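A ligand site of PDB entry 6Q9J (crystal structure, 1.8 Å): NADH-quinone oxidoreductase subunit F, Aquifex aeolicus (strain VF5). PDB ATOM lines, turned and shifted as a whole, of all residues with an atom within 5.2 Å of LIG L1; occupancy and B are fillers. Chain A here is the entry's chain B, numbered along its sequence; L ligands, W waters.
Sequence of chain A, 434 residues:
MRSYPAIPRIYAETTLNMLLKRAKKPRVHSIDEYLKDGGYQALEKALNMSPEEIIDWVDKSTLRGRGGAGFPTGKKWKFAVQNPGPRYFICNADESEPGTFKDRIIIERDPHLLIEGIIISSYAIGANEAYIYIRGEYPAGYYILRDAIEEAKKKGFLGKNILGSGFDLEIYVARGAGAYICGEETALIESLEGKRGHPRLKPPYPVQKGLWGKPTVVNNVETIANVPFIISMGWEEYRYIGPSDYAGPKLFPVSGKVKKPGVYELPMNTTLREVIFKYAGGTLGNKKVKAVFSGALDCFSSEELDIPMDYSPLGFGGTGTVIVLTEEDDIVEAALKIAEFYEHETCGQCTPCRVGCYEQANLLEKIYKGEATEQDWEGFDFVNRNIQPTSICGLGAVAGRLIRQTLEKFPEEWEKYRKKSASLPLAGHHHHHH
An oxygen (O4) of LIG L1 sits at hydrogen-bond distance from an oxygen (O9) of LG2 L2, 2.7 Å away.
The backbone carbonyl oxygen of Gly 183 sits close to a nitrogen (N4) of LIG L1. CA of Gly 65 touches O7 of LIG L1, at 3.2 Å. Asp 94 touches LIG L1. Ser 96 touches LIG L1 (N to O2, 3.8 Å). Tyr 180 touches LIG L1. Ile 181 touches LIG L1. Glu 184 touches LIG L1 (N to C4, 3.4 Å). Val 218 touches LIG L1 (O to O6, 3.6 Å). CA of Gly 394 touches C9 of LIG L1 (3.7 Å). Leu 395 touches LIG L1 (N to C9, 3.9 Å).
The side-chain hydroxyl (OG1) of Thr 223 sits at hydrogen-bond distance from the backbone NH (N) of Arg 66 (2.8 Å). ND2 of Asn 219 lies close to NZ of Lys 76 (3.5 Å). N of Asp 103 lies within hydrogen-bond range of OE2 of Glu 95 (2.8 Å). O of Gly 183 lies within hydrogen-bond range of ND2 of Asn 92 (2.7 Å). The backbone carbonyl oxygen (O) of Phe 71 is in hydrogen-bond range of the backbone NH (N) of Gly 65. N of Gly 70 is in hydrogen-bond range of O of Gly 65, 3.1 Å away. The backbone NH of Gly 183 sits at hydrogen-bond distance from the side-chain carboxylate of Asp 94, 3.1 Å away. The side-chain hydroxyl (OG) of Ser 96 lies within hydrogen-bond range of the backbone carbonyl oxygen (O) of Asp 94.
The side-chain hydroxyl (OG1) of Thr 223 sits at hydrogen-bond distance from an oxygen (O9) of LIG L1, at 2.7 Å. The side-chain amino group (NZ) of Lys 76 lies within salt-bridge range of an oxygen (O8) of LIG L1, at 2.8 Å. An oxygen (O7) of LIG L1 sits at hydrogen-bond distance from the backbone NH (N) of Gly 67. ND2 of Asn 219 is in hydrogen-bond range of O9 of LIG L1 (2.8 Å). An oxygen (O9) of LIG L1 sits at hydrogen-bond distance from the backbone NH (N) of Asn 220 (3.0 Å). The side-chain amide nitrogen of Asn 220 sits at hydrogen-bond distance from an oxygen (O1) of LIG L1 (2.8 Å). N of Glu 95 is in hydrogen-bond range of O2 of LIG L1. The backbone NH (N) of Glu 185 is in hydrogen-bond range of an oxygen (O3) of LIG L1, 3.1 Å away. The side-chain amide nitrogen (ND2) of Asn 92 lies close to an oxygen (O5) of LIG L1. The backbone NH of Arg 66 sits at hydrogen-bond distance from an oxygen (O7) of LIG L1. O5 of LG2 L2 lies within hydrogen-bond range of NZ of Lys 76 (2.8 Å). The backbone carbonyl oxygen (O) of Gly 67 sits close to a nitrogen (N7) of LG2 L2, 3.3 Å away. The side-chain carboxylate (OE2) of Glu 185 is in hydrogen-bond range of an oxygen (O6) of LG2 L2 (2.4 Å). N of Ser 96 is in hydrogen-bond range of O14 of LG2 L2 (3.0 Å). An oxygen (O12) of LG2 L2 lies within hydrogen-bond range of the backbone carbonyl oxygen (O) of Gly 68 (3.3 Å).
Water W1 lies within hydrogen-bond range of an oxygen (O8) of LIG L1 (2.7 Å), the backbone carbonyl oxygen (O) of Phe 71 (2.8 Å), the side-chain hydroxyl (OG1) of Thr 73 (2.9 Å), the side-chain amide nitrogen (ND2) of Asn 219 (3.2 Å) and the backbone NH (N) of Gly 65 (3.4 Å). Water W2 lies within hydrogen-bond range of O7 of LIG L1 (2.7 Å), N of Ala 69 (2.9 Å) and N of Gly 68 (3.3 Å). Water W4 lies within hydrogen-bond range of O8 of LIG L1 (2.7 Å), N of Phe 71 (2.9 Å) and N of Gly 70 (3.5 Å).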
ATOM      1  N   GLY A  65      17.768  20.212  17.269  1.00  0.00           N
ATOM      2  CA  GLY A  65      16.752  21.225  16.912  1.00  0.00           C
ATOM      3  C   GLY A  65      16.105  21.825  18.146  1.00  0.00           C
ATOM      4  O   GLY A  65      15.374  21.109  18.858  1.00  0.00           O
ATOM      5  N   ARG A  66      16.330  23.122  18.349  1.00  0.00           N
ATOM      6  CA  ARG A  66      15.823  23.902  19.515  1.00  0.00           C
ATOM      7  C   ARG A  66      14.371  24.341  19.270  1.00  0.00           C
ATOM      8  O   ARG A  66      13.766  24.889  20.208  1.00  0.00           O
ATOM      9  CB  ARG A  66      16.726  25.116  19.751  1.00  0.00           C
ATOM     10  CG  ARG A  66      18.186  24.761  20.028  1.00  0.00           C
ATOM     11  CD  ARG A  66      18.359  23.888  21.251  1.00  0.00           C
ATOM     12  NE  ARG A  66      19.710  23.963  21.806  1.00  0.00           N
ATOM     13  CZ  ARG A  66      20.586  22.966  21.902  1.00  0.00           C
ATOM     14  NH1 ARG A  66      21.760  23.182  22.458  1.00  0.00           N
ATOM     15  NH2 ARG A  66      20.307  21.748  21.463  1.00  0.00           N
ATOM     16  N   GLY A  67      13.829  24.093  18.077  1.00  0.00           N
ATOM     17  CA  GLY A  67      12.416  24.374  17.737  1.00  0.00           C
ATOM     18  C   GLY A  67      11.457  23.556  18.583  1.00  0.00           C
ATOM     19  O   GLY A  67      10.310  23.992  18.759  1.00  0.00           O
ATOM     20  N   GLY A  68      11.899  22.393  19.077  1.00  0.00           N
ATOM     21  CA  GLY A  68      11.125  21.557  20.017  1.00  0.00           C
ATOM     22  C   GLY A  68      11.197  20.063  19.728  1.00  0.00           C
ATOM     23  O   GLY A  68      10.956  19.293  20.673  1.00  0.00           O
ATOM     24  N   ALA A  69      11.490  19.651  18.489  1.00  0.00           N
ATOM     25  CA  ALA A  69      11.530  18.220  18.117  1.00  0.00           C
ATOM     26  C   ALA A  69      12.902  17.614  18.446  1.00  0.00           C
ATOM     27  O   ALA A  69      12.966  16.381  18.598  1.00  0.00           O
ATOM     28  CB  ALA A  69      11.164  18.023  16.660  1.00  0.00           C
ATOM     29  N   GLY A  70      13.955  18.424  18.541  1.00  0.00           N
ATOM     30  CA  GLY A  70      15.317  17.965  18.912  1.00  0.00           C
ATOM     31  C   GLY A  70      15.976  17.095  17.851  1.00  0.00           C
ATOM     32  O   GLY A  70      16.806  16.248  18.226  1.00  0.00           O
ATOM     33  N   PHE A  71      15.673  17.303  16.564  1.00  0.00           N
ATOM     34  CA  PHE A  71      16.322  16.556  15.459  1.00  0.00           C
ATOM     35  C   PHE A  71      17.793  16.976  15.347  1.00  0.00           C
ATOM     36  O   PHE A  71      18.095  18.167  15.403  1.00  0.00           O
ATOM     37  CB  PHE A  71      15.579  16.749  14.141  1.00  0.00           C
ATOM     38  CG  PHE A  71      15.980  15.763  13.092  1.00  0.00           C
ATOM     39  CD1 PHE A  71      15.343  14.538  12.987  1.00  0.00           C
ATOM     40  CD2 PHE A  71      17.036  16.036  12.233  1.00  0.00           C
ATOM     41  CE1 PHE A  71      15.730  13.616  12.027  1.00  0.00           C
ATOM     42  CE2 PHE A  71      17.428  15.106  11.276  1.00  0.00           C
ATOM     43  CZ  PHE A  71      16.766  13.902  11.169  1.00  0.00           C
ATOM     44  N   THR A  73      20.983  18.496  14.174  1.00  0.00           N
ATOM     45  CA  THR A  73      21.101  19.594  13.178  1.00  0.00           C
ATOM     46  C   THR A  73      22.072  19.203  12.054  1.00  0.00           C
ATOM     47  O   THR A  73      21.726  19.372  10.870  1.00  0.00           O
ATOM     48  CB  THR A  73      21.487  20.908  13.879  1.00  0.00           C
ATOM     49  OG1 THR A  73      20.580  21.124  14.964  1.00  0.00           O
ATOM     50  CG2 THR A  73      21.439  22.098  12.935  1.00  0.00           C
ATOM     51  N   LYS A  76      20.502  16.746   9.715  1.00  0.00           N
ATOM     52  CA  LYS A  76      19.533  17.419   8.817  1.00  0.00           C
ATOM     53  C   LYS A  76      20.290  18.025   7.630  1.00  0.00           C
ATOM     54  O   LYS A  76      19.883  17.777   6.475  1.00  0.00           O
ATOM     55  CB  LYS A  76      18.715  18.497   9.553  1.00  0.00           C
ATOM     56  CG  LYS A  76      17.516  19.018   8.780  1.00  0.00           C
ATOM     57  CD  LYS A  76      16.847  20.232   9.400  1.00  0.00           C
ATOM     58  CE  LYS A  76      16.258  19.960  10.764  1.00  0.00           C
ATOM     59  NZ  LYS A  76      15.304  21.020  11.156  1.00  0.00           N
ATOM     60  N   ASN A  92      13.334  29.706  11.047  1.00  0.00           N
ATOM     61  CA  ASN A  92      11.952  29.662  11.584  1.00  0.00           C
ATOM     62  C   ASN A  92      11.878  30.574  12.804  1.00  0.00           C
ATOM     63  O   ASN A  92      12.367  30.169  13.879  1.00  0.00           O
ATOM     64  CB  ASN A  92      11.513  28.233  11.918  1.00  0.00           C
ATOM     65  CG  ASN A  92      10.019  28.127  12.156  1.00  0.00           C
ATOM     66  OD1 ASN A  92       9.369  29.129  12.446  1.00  0.00           O
ATOM     67  ND2 ASN A  92       9.471  26.938  12.023  1.00  0.00           N
ATOM     68  N   ASP A  94       8.725  31.833  13.738  1.00  0.00           N
ATOM     69  CA  ASP A  94       7.243  31.904  13.884  1.00  0.00           C
ATOM     70  C   ASP A  94       6.826  31.749  15.351  1.00  0.00           C
ATOM     71  O   ASP A  94       5.633  31.993  15.627  1.00  0.00           O
ATOM     72  CB  ASP A  94       6.515  30.888  13.013  1.00  0.00           C
ATOM     73  CG  ASP A  94       5.080  31.314  12.776  1.00  0.00           C
ATOM     74  OD1 ASP A  94       4.914  32.416  12.223  1.00  0.00           O
ATOM     75  OD2 ASP A  94       4.161  30.578  13.186  1.00  0.00           O
ATOM     76  N   GLU A  95       7.746  31.374  16.244  1.00  0.00           N
ATOM     77  CA  GLU A  95       7.555  31.160  17.706  1.00  0.00           C
ATOM     78  C   GLU A  95       6.149  31.567  18.163  1.00  0.00           C
ATOM     79  O   GLU A  95       5.928  32.774  18.402  1.00  0.00           O
ATOM     80  CB  GLU A  95       8.616  31.935  18.476  1.00  0.00           C
ATOM     81  CG  GLU A  95       8.480  31.784  19.981  1.00  0.00           C
ATOM     82  CD  GLU A  95       9.672  32.312  20.746  1.00  0.00           C
ATOM     83  OE1 GLU A  95       9.899  33.543  20.712  1.00  0.00           O
ATOM     84  OE2 GLU A  95      10.400  31.486  21.337  1.00  0.00           O
ATOM     85  N   SER A  96       5.254  30.597  18.322  1.00  0.00           N
ATOM     86  CA  SER A  96       3.829  30.831  18.693  1.00  0.00           C
ATOM     87  C   SER A  96       3.304  29.794  19.701  1.00  0.00           C
ATOM     88  O   SER A  96       2.129  29.905  20.048  1.00  0.00           O
ATOM     89  CB  SER A  96       2.961  30.869  17.459  1.00  0.00           C
ATOM     90  OG  SER A  96       3.343  31.933  16.604  1.00  0.00           O
ATOM     91  N   ASP A 103      12.935  32.643  21.614  1.00  0.00           N
ATOM     92  CA  ASP A 103      13.531  33.078  20.320  1.00  0.00           C
ATOM     93  C   ASP A 103      13.522  34.603  20.197  1.00  0.00           C
ATOM     94  O   ASP A 103      14.495  35.171  19.667  1.00  0.00           O
ATOM     95  CB  ASP A 103      12.814  32.482  19.112  1.00  0.00           C
ATOM     96  CG  ASP A 103      12.871  30.963  19.048  1.00  0.00           C
ATOM     97  OD1 ASP A 103      13.724  30.382  19.747  1.00  0.00           O
ATOM     98  OD2 ASP A 103      12.060  30.384  18.313  1.00  0.00           O
ATOM     99  N   TYR A 180      -0.623  30.006  13.802  1.00  0.00           N
ATOM    100  CA  TYR A 180       0.285  29.080  14.534  1.00  0.00           C
ATOM    101  C   TYR A 180       0.844  28.026  13.571  1.00  0.00           C
ATOM    102  O   TYR A 180       2.019  27.651  13.722  1.00  0.00           O
ATOM    103  CB  TYR A 180      -0.508  28.429  15.664  1.00  0.00           C
ATOM    104  CG  TYR A 180       0.127  27.267  16.386  1.00  0.00           C
ATOM    105  CD1 TYR A 180       1.153  27.441  17.306  1.00  0.00           C
ATOM    106  CD2 TYR A 180      -0.401  25.994  16.244  1.00  0.00           C
ATOM    107  CE1 TYR A 180       1.666  26.378  18.023  1.00  0.00           C
ATOM    108  CE2 TYR A 180       0.112  24.916  16.951  1.00  0.00           C
ATOM    109  CZ  TYR A 180       1.141  25.106  17.838  1.00  0.00           C
ATOM    110  OH  TYR A 180       1.618  24.031  18.539  1.00  0.00           O
ATOM    111  N   ILE A 181       0.017  27.536  12.648  1.00  0.00           N
ATOM    112  CA  ILE A 181       0.351  26.389  11.766  1.00  0.00           C
ATOM    113  C   ILE A 181       1.498  26.768  10.831  1.00  0.00           C
ATOM    114  O   ILE A 181       2.188  25.862  10.357  1.00  0.00           O
ATOM    115  CB  ILE A 181      -0.898  25.868  11.007  1.00  0.00           C
ATOM    116  CG1 ILE A 181      -0.625  24.519  10.339  1.00  0.00           C
ATOM    117  CG2 ILE A 181      -1.423  26.893  10.013  1.00  0.00           C
ATOM    118  CD1 ILE A 181      -0.023  23.487  11.247  1.00  0.00           C
ATOM    119  N   GLY A 183       4.250  27.954  11.510  1.00  0.00           N
ATOM    120  CA  GLY A 183       5.519  27.527  12.122  1.00  0.00           C
ATOM    121  C   GLY A 183       5.866  26.088  11.777  1.00  0.00           C
ATOM    122  O   GLY A 183       7.057  25.719  11.880  1.00  0.00           O
ATOM    123  N   GLU A 184       4.878  25.278  11.404  1.00  0.00           N
ATOM    124  CA  GLU A 184       5.127  23.920  10.868  1.00  0.00           C
ATOM    125  C   GLU A 184       5.916  24.114   9.564  1.00  0.00           C
ATOM    126  O   GLU A 184       5.485  24.943   8.733  1.00  0.00           O
ATOM    127  CB  GLU A 184       3.824  23.144  10.692  1.00  0.00           C
ATOM    128  CG  GLU A 184       4.015  21.636  10.589  1.00  0.00           C
ATOM    129  CD  GLU A 184       4.390  21.109   9.206  1.00  0.00           C
ATOM    130  OE1 GLU A 184       4.409  21.909   8.238  1.00  0.00           O
ATOM    131  OE2 GLU A 184       4.619  19.898   9.103  1.00  0.00           O
ATOM    132  N   GLU A 185       7.056  23.443   9.431  1.00  0.00           N
ATOM    133  CA  GLU A 185       8.097  23.803   8.417  1.00  0.00           C
ATOM    134  C   GLU A 185       7.504  23.780   7.003  1.00  0.00           C
ATOM    135  O   GLU A 185       7.914  24.629   6.195  1.00  0.00           O
ATOM    136  CB  GLU A 185       9.309  22.879   8.528  1.00  0.00           C
ATOM    137  CG  GLU A 185       8.988  21.412   8.391  1.00  0.00           C
ATOM    138  CD  GLU A 185      10.191  20.493   8.453  1.00  0.00           C
ATOM    139  OE1 GLU A 185      11.308  21.000   8.671  1.00  0.00           O
ATOM    140  OE2 GLU A 185      10.007  19.279   8.265  1.00  0.00           O
ATOM    141  N   VAL A 218      15.115  23.896   7.148  1.00  0.00           N
ATOM    142  CA  VAL A 218      14.403  24.779   8.107  1.00  0.00           C
ATOM    143  C   VAL A 218      15.030  24.539   9.475  1.00  0.00           C
ATOM    144  O   VAL A 218      15.097  23.362   9.900  1.00  0.00           O
ATOM    145  CB  VAL A 218      12.881  24.524   8.122  1.00  0.00           C
ATOM    146  CG1 VAL A 218      12.179  25.462   9.093  1.00  0.00           C
ATOM    147  CG2 VAL A 218      12.287  24.655   6.720  1.00  0.00           C
ATOM    148  N   ASN A 219      15.511  25.605  10.112  1.00  0.00           N
ATOM    149  CA  ASN A 219      16.037  25.552  11.501  1.00  0.00           C
ATOM    150  C   ASN A 219      15.450  26.697  12.304  1.00  0.00           C
ATOM    151  O   ASN A 219      15.174  27.777  11.747  1.00  0.00           O
ATOM    152  CB  ASN A 219      17.569  25.565  11.559  1.00  0.00           C
ATOM    153  CG  ASN A 219      18.172  24.180  11.392  1.00  0.00           C
ATOM    154  OD1 ASN A 219      19.005  23.994  10.502  1.00  0.00           O
ATOM    155  ND2 ASN A 219      17.774  23.239  12.221  1.00  0.00           N
ATOM    156  N   ASN A 220      15.248  26.424  13.578  1.00  0.00           N
ATOM    157  CA  ASN A 220      14.739  27.360  14.603  1.00  0.00           C
ATOM    158  C   ASN A 220      15.811  28.415  14.912  1.00  0.00           C
ATOM    159  O   ASN A 220      17.012  28.097  14.852  1.00  0.00           O
ATOM    160  CB  ASN A 220      14.328  26.565  15.846  1.00  0.00           C
ATOM    161  CG  ASN A 220      13.981  27.433  17.035  1.00  0.00           C
ATOM    162  OD1 ASN A 220      14.795  27.598  17.937  1.00  0.00           O
ATOM    163  ND2 ASN A 220      12.775  27.983  17.025  1.00  0.00           N
ATOM    164  N   VAL A 221      15.362  29.633  15.235  1.00  0.00           N
ATOM    165  CA  VAL A 221      16.186  30.796  15.680  1.00  0.00           C
ATOM    166  C   VAL A 221      17.253  30.318  16.677  1.00  0.00           C
ATOM    167  O   VAL A 221      18.460  30.580  16.444  1.00  0.00           O
ATOM    168  CB  VAL A 221      15.301  31.890  16.309  1.00  0.00           C
ATOM    169  CG1 VAL A 221      16.127  32.924  17.069  1.00  0.00           C
ATOM    170  CG2 VAL A 221      14.410  32.566  15.280  1.00  0.00           C
ATOM    171  N   THR A 223      18.404  27.311  17.481  1.00  0.00           N
ATOM    172  CA  THR A 223      19.341  26.343  16.835  1.00  0.00           C
ATOM    173  C   THR A 223      20.436  27.126  16.107  1.00  0.00           C
ATOM    174  O   THR A 223      21.632  26.857  16.349  1.00  0.00           O
ATOM    175  CB  THR A 223      18.629  25.402  15.869  1.00  0.00           C
ATOM    176  OG1 THR A 223      17.484  24.849  16.518  1.00  0.00           O
ATOM    177  CG2 THR A 223      19.539  24.300  15.372  1.00  0.00           C
ATOM    178  N   CYS A 393       0.417  16.460   9.921  1.00  0.00           N
ATOM    179  CA  CYS A 393       1.401  17.292  10.665  1.00  0.00           C
ATOM    180  C   CYS A 393       1.234  17.106  12.180  1.00  0.00           C
ATOM    181  O   CYS A 393       0.272  16.446  12.610  1.00  0.00           O
ATOM    182  CB  CYS A 393       1.332  18.763  10.255  1.00  0.00           C
ATOM    183  SG  CYS A 393       0.239  19.793  11.277  1.00  0.00           S
ATOM    184  N   GLY A 394       2.181  17.655  12.933  1.00  0.00           N
ATOM    185  CA  GLY A 394       2.324  17.471  14.389  1.00  0.00           C
ATOM    186  C   GLY A 394       1.154  18.023  15.173  1.00  0.00           C
ATOM    187  O   GLY A 394       0.992  17.557  16.312  1.00  0.00           O
ATOM    188  N   LEU A 395       0.385  18.973  14.645  1.00  0.00           N
ATOM    189  CA  LEU A 395      -0.740  19.626  15.378  1.00  0.00           C
ATOM    190  C   LEU A 395      -1.806  18.554  15.686  1.00  0.00           C
ATOM    191  O   LEU A 395      -2.100  18.339  16.883  1.00  0.00           O
ATOM    192  CB  LEU A 395      -1.306  20.783  14.555  1.00  0.00           C
ATOM    193  CG  LEU A 395      -2.242  21.744  15.300  1.00  0.00           C
ATOM    194  CD1 LEU A 395      -2.243  23.115  14.663  1.00  0.00           C
ATOM    195  CD2 LEU A 395      -3.668  21.197  15.375  1.00  0.00           C
HETATM  196  N1  LIG L   1       9.432  25.328  14.860  1.00  0.00           N
HETATM  197  C1  LIG L   1       9.917  26.569  15.127  1.00  0.00           C
HETATM  198  O1  LIG L   1      11.130  26.796  15.085  1.00  0.00           O
HETATM  199  N2  LIG L   1       9.037  27.618  15.387  1.00  0.00           N
HETATM  200  C2  LIG L   1       7.667  27.538  15.372  1.00  0.00           C
HETATM  201  O2  LIG L   1       6.985  28.536  15.626  1.00  0.00           O
HETATM  202  C3  LIG L   1       7.152  26.212  15.064  1.00  0.00           C
HETATM  203  N3  LIG L   1       5.859  26.050  14.989  1.00  0.00           N
HETATM  204  C4  LIG L   1       5.375  24.767  14.692  1.00  0.00           C
HETATM  205  C5  LIG L   1       3.998  24.552  14.627  1.00  0.00           C
HETATM  206  C6  LIG L   1       3.469  23.291  14.407  1.00  0.00           C
HETATM  207  C7  LIG L   1       1.976  23.106  14.365  1.00  0.00           C
HETATM  208  C8  LIG L   1       4.342  22.202  14.223  1.00  0.00           C
HETATM  209  C9  LIG L   1       3.823  20.797  14.048  1.00  0.00           C
HETATM  210  C10 LIG L   1       5.715  22.413  14.242  1.00  0.00           C
HETATM  211  C11 LIG L   1       6.245  23.680  14.484  1.00  0.00           C
HETATM  212  N4  LIG L   1       7.645  23.918  14.547  1.00  0.00           N
HETATM  213  C12 LIG L   1       8.118  25.168  14.830  1.00  0.00           C
HETATM  214  C13 LIG L   1       8.624  22.858  14.277  1.00  0.00           C
HETATM  215  C14 LIG L   1       9.080  22.863  12.824  1.00  0.00           C
HETATM  216  O3  LIG L   1       8.170  22.110  12.022  1.00  0.00           O
HETATM  217  C15 LIG L   1      10.498  22.304  12.666  1.00  0.00           C
HETATM  218  O4  LIG L   1      10.601  21.051  13.331  1.00  0.00           O
HETATM  219  C16 LIG L   1      11.630  23.200  13.165  1.00  0.00           C
HETATM  220  O5  LIG L   1      11.414  24.554  12.773  1.00  0.00           O
HETATM  221  C17 LIG L   1      12.959  22.685  12.669  1.00  0.00           C
HETATM  222  O6  LIG L   1      14.021  23.417  13.288  1.00  0.00           O
HETATM  223  P1  LIG L   1      14.964  22.781  14.403  1.00  0.00           P
HETATM  224  O7  LIG L   1      14.208  22.681  15.694  1.00  0.00           O
HETATM  225  O8  LIG L   1      15.439  21.406  13.892  1.00  0.00           O
HETATM  226  O9  LIG L   1      16.175  23.712  14.474  1.00  0.00           O
HETATM  227  P1  LG2 L   2       9.574  16.226  13.540  1.00  0.00           P
HETATM  228  O1  LG2 L   2      10.161  15.399  14.627  1.00  0.00           O
HETATM  229  O2  LG2 L   2       8.613  15.515  12.614  1.00  0.00           O
HETATM  230  O3  LG2 L   2      10.714  16.906  12.618  1.00  0.00           O
HETATM  231  C1  LG2 L   2      11.748  17.712  13.220  1.00  0.00           C
HETATM  232  C2  LG2 L   2      12.719  18.173  12.158  1.00  0.00           C
HETATM  233  O4  LG2 L   2      13.507  17.057  11.707  1.00  0.00           O
HETATM  234  C3  LG2 L   2      12.082  18.789  10.907  1.00  0.00           C
HETATM  235  O5  LG2 L   2      12.887  19.832  10.396  1.00  0.00           O
HETATM  236  C4  LG2 L   2      12.022  17.581   9.951  1.00  0.00           C
HETATM  237  O6  LG2 L   2      12.047  17.979   8.580  1.00  0.00           O
HETATM  238  C5  LG2 L   2      13.313  16.862  10.316  1.00  0.00           C
HETATM  239  N1  LG2 L   2      13.277  15.424  10.052  1.00  0.00           N
HETATM  240  C6  LG2 L   2      12.596  14.461  10.745  1.00  0.00           C
HETATM  241  N2  LG2 L   2      12.714  13.253  10.241  1.00  0.00           N
HETATM  242  C7  LG2 L   2      13.520  13.431   9.132  1.00  0.00           C
HETATM  243  C8  LG2 L   2      14.020  12.539   8.156  1.00  0.00           C
HETATM  244  N3  LG2 L   2      13.738  11.230   8.137  1.00  0.00           N
HETATM  245  N4  LG2 L   2      14.802  13.045   7.182  1.00  0.00           N
HETATM  246  C9  LG2 L   2      15.075  14.357   7.186  1.00  0.00           C
HETATM  247  N5  LG2 L   2      14.659  15.293   8.044  1.00  0.00           N
HETATM  248  C10 LG2 L   2      13.886  14.764   9.001  1.00  0.00           C
HETATM  249  O7  LG2 L   2       8.791  17.454  14.174  1.00  0.00           O
HETATM  250  P2  LG2 L   2       7.899  18.630  13.599  1.00  0.00           P
HETATM  251  O8  LG2 L   2       6.526  18.062  13.304  1.00  0.00           O
HETATM  252  O9  LG2 L   2       8.568  19.406  12.517  1.00  0.00           O
HETATM  253  O10 LG2 L   2       7.767  19.544  14.926  1.00  0.00           O
HETATM  254  C11 LG2 L   2       7.120  19.170  16.160  1.00  0.00           C
HETATM  255  C12 LG2 L   2       7.613  20.073  17.261  1.00  0.00           C
HETATM  256  O11 LG2 L   2       7.253  21.443  16.980  1.00  0.00           O
HETATM  257  C13 LG2 L   2       7.048  19.785  18.648  1.00  0.00           C
HETATM  258  O12 LG2 L   2       7.956  18.976  19.384  1.00  0.00           O
HETATM  259  C14 LG2 L   2       6.884  21.173  19.297  1.00  0.00           C
HETATM  260  O13 LG2 L   2       7.684  21.303  20.470  1.00  0.00           O
HETATM  261  C15 LG2 L   2       7.399  22.136  18.212  1.00  0.00           C
HETATM  262  N6  LG2 L   2       6.673  23.399  18.134  1.00  0.00           N
HETATM  263  C16 LG2 L   2       7.302  24.628  18.466  1.00  0.00           C
HETATM  264  C17 LG2 L   2       6.677  25.812  18.416  1.00  0.00           C
HETATM  265  C18 LG2 L   2       7.425  27.027  18.813  1.00  0.00           C
HETATM  266  O14 LG2 L   2       6.818  28.090  18.998  1.00  0.00           O
HETATM  267  N7  LG2 L   2       8.741  26.931  18.957  1.00  0.00           N
HETATM  268  C19 LG2 L   2       5.247  25.897  17.992  1.00  0.00           C
HETATM  269  C20 LG2 L   2       4.679  24.556  17.683  1.00  0.00           C
HETATM  270  C21 LG2 L   2       5.367  23.434  17.758  1.00  0.00           C
HETATM  271  O   HOH W   1      17.954  20.456  13.884  1.00  0.00           O
HETATM  272  O   HOH W   2      12.038  21.108  15.987  1.00  0.00           O
HETATM  273  O   HOH W   3       4.196  28.660  15.218  1.00  0.00           O
HETATM  274  O   HOH W   4      14.191  19.411  15.235  1.00  0.00           O
HETATM  275  O   HOH W   5      10.491  30.175  16.090  1.00  0.00           O
